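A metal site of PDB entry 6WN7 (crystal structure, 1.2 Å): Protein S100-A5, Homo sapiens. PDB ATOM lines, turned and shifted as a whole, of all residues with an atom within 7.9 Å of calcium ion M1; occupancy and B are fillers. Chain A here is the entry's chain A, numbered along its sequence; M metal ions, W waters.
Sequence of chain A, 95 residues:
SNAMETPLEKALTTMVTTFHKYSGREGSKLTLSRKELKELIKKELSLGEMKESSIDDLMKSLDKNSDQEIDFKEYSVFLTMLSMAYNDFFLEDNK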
ATOM      1  N   THR A  31     -30.381  25.103 -26.292  1.00  0.00           N
ATOM      2  CA  THR A  31     -29.261  25.688 -27.007  1.00  0.00           C
ATOM      3  C   THR A  31     -29.133  25.051 -28.371  1.00  0.00           C
ATOM      4  O   THR A  31     -29.563  23.923 -28.598  1.00  0.00           O
ATOM      5  CB  THR A  31     -27.952  25.506 -26.248  1.00  0.00           C
ATOM      6  OG1 THR A  31     -27.743  24.099 -26.022  1.00  0.00           O
ATOM      7  CG2 THR A  31     -27.986  26.247 -24.934  1.00  0.00           C
ATOM      8  N   LEU A  32     -28.495  25.803 -29.269  1.00  0.00           N
ATOM      9  CA  LEU A  32     -28.124  25.329 -30.595  1.00  0.00           C
ATOM     10  C   LEU A  32     -26.656  24.897 -30.593  1.00  0.00           C
ATOM     11  O   LEU A  32     -25.768  25.688 -30.253  1.00  0.00           O
ATOM     12  CB  LEU A  32     -28.305  26.447 -31.609  1.00  0.00           C
ATOM     13  CG  LEU A  32     -29.679  27.084 -31.773  1.00  0.00           C
ATOM     14  CD1 LEU A  32     -29.520  28.468 -32.290  1.00  0.00           C
ATOM     15  CD2 LEU A  32     -30.495  26.284 -32.706  1.00  0.00           C
ATOM     16  N   MET A  59     -19.968  30.945 -35.319  1.00  0.00           N
ATOM     17  CA  MET A  59     -20.172  30.199 -34.100  1.00  0.00           C
ATOM     18  C   MET A  59     -19.370  30.781 -32.945  1.00  0.00           C
ATOM     19  O   MET A  59     -19.878  30.952 -31.836  1.00  0.00           O
ATOM     20  CB  MET A  59     -19.782  28.749 -34.354  1.00  0.00           C
ATOM     21  CG  MET A  59     -20.199  27.824 -33.271  1.00  0.00           C
ATOM     22  SD  MET A  59     -21.964  27.659 -33.123  1.00  0.00           S
ATOM     23  CE  MET A  59     -22.037  26.903 -31.509  1.00  0.00           C
ATOM     24  N   LEU A  62     -20.411  34.274 -31.570  1.00  0.00           N
ATOM     25  CA  LEU A  62     -21.690  34.258 -30.871  1.00  0.00           C
ATOM     26  C   LEU A  62     -21.584  33.632 -29.486  1.00  0.00           C
ATOM     27  O   LEU A  62     -22.402  33.928 -28.610  1.00  0.00           O
ATOM     28  CB  LEU A  62     -22.693  33.425 -31.665  1.00  0.00           C
ATOM     29  CG  LEU A  62     -23.262  34.027 -32.935  1.00  0.00           C
ATOM     30  CD1 LEU A  62     -24.200  32.982 -33.501  1.00  0.00           C
ATOM     31  CD2 LEU A  62     -23.957  35.343 -32.692  1.00  0.00           C
ATOM     32  N   ASP A  63     -20.601  32.766 -29.286  1.00  0.00           N
ATOM     33  CA  ASP A  63     -20.557  31.903 -28.111  1.00  0.00           C
ATOM     34  C   ASP A  63     -19.815  32.580 -26.959  1.00  0.00           C
ATOM     35  O   ASP A  63     -18.829  32.078 -26.441  1.00  0.00           O
ATOM     36  CB  ASP A  63     -19.911  30.580 -28.482  1.00  0.00           C
ATOM     37  CG  ASP A  63     -20.019  29.587 -27.394  1.00  0.00           C
ATOM     38  OD1 ASP A  63     -20.810  29.814 -26.473  1.00  0.00           O
ATOM     39  OD2 ASP A  63     -19.288  28.585 -27.458  1.00  0.00           O
ATOM     40  N   LYS A  64     -20.375  33.716 -26.528  1.00  0.00           N
ATOM     41  CA  LYS A  64     -19.731  34.589 -25.556  1.00  0.00           C
ATOM     42  C   LYS A  64     -19.300  33.881 -24.276  1.00  0.00           C
ATOM     43  O   LYS A  64     -18.325  34.296 -23.650  1.00  0.00           O
ATOM     44  CB  LYS A  64     -20.676  35.739 -25.208  1.00  0.00           C
ATOM     45  N   ASN A  65     -20.001  32.833 -23.841  1.00  0.00           N
ATOM     46  CA  ASN A  65     -19.570  32.073 -22.677  1.00  0.00           C
ATOM     47  C   ASN A  65     -18.646  30.913 -23.019  1.00  0.00           C
ATOM     48  O   ASN A  65     -18.219  30.206 -22.112  1.00  0.00           O
ATOM     49  CB  ASN A  65     -20.776  31.561 -21.884  1.00  0.00           C
ATOM     50  CG  ASN A  65     -21.579  30.573 -22.661  1.00  0.00           C
ATOM     51  OD1 ASN A  65     -21.421  30.415 -23.862  1.00  0.00           O
ATOM     52  ND2 ASN A  65     -22.471  29.890 -21.979  1.00  0.00           N
ATOM     53  N   SER A  66     -18.353  30.699 -24.292  1.00  0.00           N
ATOM     54  CA  SER A  66     -17.406  29.701 -24.758  1.00  0.00           C
ATOM     55  C   SER A  66     -17.824  28.270 -24.432  1.00  0.00           C
ATOM     56  O   SER A  66     -16.993  27.374 -24.433  1.00  0.00           O
ATOM     57  CB  SER A  66     -16.000  30.019 -24.236  1.00  0.00           C
ATOM     58  OG  SER A  66     -15.284  30.832 -25.162  1.00  0.00           O
ATOM     59  N   ASP A  67     -19.116  28.010 -24.225  1.00  0.00           N
ATOM     60  CA  ASP A  67     -19.584  26.687 -23.865  1.00  0.00           C
ATOM     61  C   ASP A  67     -19.871  25.790 -25.056  1.00  0.00           C
ATOM     62  O   ASP A  67     -20.373  24.683 -24.882  1.00  0.00           O
ATOM     63  CB  ASP A  67     -20.807  26.765 -22.952  1.00  0.00           C
ATOM     64  CG  ASP A  67     -22.059  27.243 -23.678  1.00  0.00           C
ATOM     65  OD1 ASP A  67     -21.961  27.851 -24.765  1.00  0.00           O
ATOM     66  OD2 ASP A  67     -23.149  27.028 -23.127  1.00  0.00           O
ATOM     67  N   GLN A  68     -19.559  26.224 -26.266  1.00  0.00           N
ATOM     68  CA  GLN A  68     -19.736  25.437 -27.479  1.00  0.00           C
ATOM     69  C   GLN A  68     -21.190  25.409 -27.958  1.00  0.00           C
ATOM     70  O   GLN A  68     -21.464  24.742 -28.947  1.00  0.00           O
ATOM     71  CB  GLN A  68     -19.219  24.003 -27.312  1.00  0.00           C
ATOM     72  CG  GLN A  68     -17.767  23.960 -26.830  1.00  0.00           C
ATOM     73  CD  GLN A  68     -16.841  24.712 -27.760  1.00  0.00           C
ATOM     74  OE1 GLN A  68     -16.260  25.737 -27.391  1.00  0.00           O
ATOM     75  NE2 GLN A  68     -16.692  24.200 -28.969  1.00  0.00           N
ATOM     76  N   GLU A  69     -22.099  26.132 -27.309  1.00  0.00           N
ATOM     77  CA  GLU A  69     -23.525  26.084 -27.614  1.00  0.00           C
ATOM     78  C   GLU A  69     -24.046  27.508 -27.718  1.00  0.00           C
ATOM     79  O   GLU A  69     -23.563  28.393 -27.017  1.00  0.00           O
ATOM     80  CB  GLU A  69     -24.304  25.413 -26.482  1.00  0.00           C
ATOM     81  CG  GLU A  69     -23.849  23.994 -26.138  1.00  0.00           C
ATOM     82  CD  GLU A  69     -24.598  22.932 -26.916  1.00  0.00           C
ATOM     83  OE1 GLU A  69     -24.229  21.738 -26.804  1.00  0.00           O
ATOM     84  OE2 GLU A  69     -25.545  23.274 -27.648  1.00  0.00           O
ATOM     85  N   ILE A  70     -25.039  27.718 -28.563  1.00  0.00           N
ATOM     86  CA  ILE A  70     -25.673  29.030 -28.688  1.00  0.00           C
ATOM     87  C   ILE A  70     -27.016  28.991 -27.955  1.00  0.00           C
ATOM     88  O   ILE A  70     -27.924  28.273 -28.361  1.00  0.00           O
ATOM     89  CB  ILE A  70     -25.836  29.440 -30.163  1.00  0.00           C
ATOM     90  CG1 ILE A  70     -24.490  29.396 -30.889  1.00  0.00           C
ATOM     91  CG2 ILE A  70     -26.417  30.842 -30.298  1.00  0.00           C
ATOM     92  CD1 ILE A  70     -23.390  30.090 -30.143  1.00  0.00           C
ATOM     93  N   ASP A  71     -27.145  29.768 -26.889  1.00  0.00           N
ATOM     94  CA  ASP A  71     -28.410  29.891 -26.175  1.00  0.00           C
ATOM     95  C   ASP A  71     -29.238  31.008 -26.791  1.00  0.00           C
ATOM     96  O   ASP A  71     -28.862  31.591 -27.814  1.00  0.00           O
ATOM     97  CB  ASP A  71     -28.220  30.061 -24.663  1.00  0.00           C
ATOM     98  CG  ASP A  71     -27.550  31.345 -24.291  1.00  0.00           C
ATOM     99  OD1 ASP A  71     -27.681  32.336 -25.040  1.00  0.00           O
ATOM    100  OD2 ASP A  71     -26.871  31.352 -23.247  1.00  0.00           O
ATOM    101  N   PHE A  72     -30.389  31.265 -26.188  1.00  0.00           N
ATOM    102  CA  PHE A  72     -31.322  32.252 -26.778  1.00  0.00           C
ATOM    103  C   PHE A  72     -30.685  33.676 -26.819  1.00  0.00           C
ATOM    104  O   PHE A  72     -30.852  34.419 -27.781  1.00  0.00           O
ATOM    105  CB  PHE A  72     -32.718  32.348 -26.107  1.00  0.00           C
ATOM    106  CG  PHE A  72     -33.637  33.309 -26.852  1.00  0.00           C
ATOM    107  CD1 PHE A  72     -34.199  32.926 -28.063  1.00  0.00           C
ATOM    108  CD2 PHE A  72     -33.850  34.587 -26.411  1.00  0.00           C
ATOM    109  CE1 PHE A  72     -34.951  33.796 -28.801  1.00  0.00           C
ATOM    110  CE2 PHE A  72     -34.632  35.414 -27.127  1.00  0.00           C
ATOM    111  CZ  PHE A  72     -35.187  34.999 -28.322  1.00  0.00           C
ATOM    112  N   GLU A  74     -27.540  34.438 -26.973  1.00  0.00           N
ATOM    113  CA  GLU A  74     -26.509  34.482 -28.009  1.00  0.00           C
ATOM    114  C   GLU A  74     -27.118  34.498 -29.410  1.00  0.00           C
ATOM    115  O   GLU A  74     -26.557  35.123 -30.311  1.00  0.00           O
ATOM    116  CB  GLU A  74     -25.550  33.281 -27.857  1.00  0.00           C
ATOM    117  CG  GLU A  74     -24.718  33.302 -26.573  1.00  0.00           C
ATOM    118  CD  GLU A  74     -23.934  32.018 -26.291  1.00  0.00           C
ATOM    119  OE1 GLU A  74     -24.390  30.952 -26.700  1.00  0.00           O
ATOM    120  OE2 GLU A  74     -22.882  32.061 -25.650  1.00  0.00           O
HETATM  121 CA    CA M   1     -22.751  29.741 -25.464  1.00  0.00          CA
HETATM  122 CA    CA M   2     -23.710  36.465 -28.880  1.00  0.00          CA
HETATM  123  O   HOH W   1     -24.394  29.298 -24.082  1.00  0.00           O
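Of the 15 residues printed, 5 come within 4 Å of calcium ion M1.
Along chain A the residues within 4 Å of calcium ion M1 span positions 63 to 74.
The nearest printed residue that does not touch calcium ion M1 is Ile 70 (4.4 Å).
Water W1 lies within hydrogen-bond range of the side-chain carboxylate of Asp 67 (2.8 Å), the side-chain amide nitrogen of Asn 65 (2.9 Å) and the side-chain carboxylate of Asp 71 (3.3 Å).
The side-chain carboxylate (OE2) of Glu 69 is in hydrogen-bond range of the side-chain hydroxyl (OG1) of Thr 31, at 2.9 Å.
The backbone NH (N) of Lys 64 lies close to the side-chain carboxylate (OE2) of Glu 74 (3.1 Å).
The side-chain carboxylate of Asp 71 sits at hydrogen-bond distance from the backbone NH of Glu 74, 2.9 Å away.
The side-chain carboxylate (OD2) of Asp 63 is in hydrogen-bond range of the backbone NH (N) of Gln 68 (2.7 Å).
The backbone NH of Ser 66 lies close to the side-chain carboxylate of Asp 63, 3.4 Å away.
Calcium ion M1 is bound by the side-chain carboxylate (OD1) of Asp 67, the side-chain amide oxygen (OD1) of Asn 65, the side-chain carboxylate (OD1) of Asp 63, water W1, the backbone carbonyl oxygen (O) of Glu 69, the side-chain carboxylate (OE2) of Glu 74 and the side-chain carboxylate (OE1) of Glu 74.
Calcium ion M1 has seven donor atoms within binding distance.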
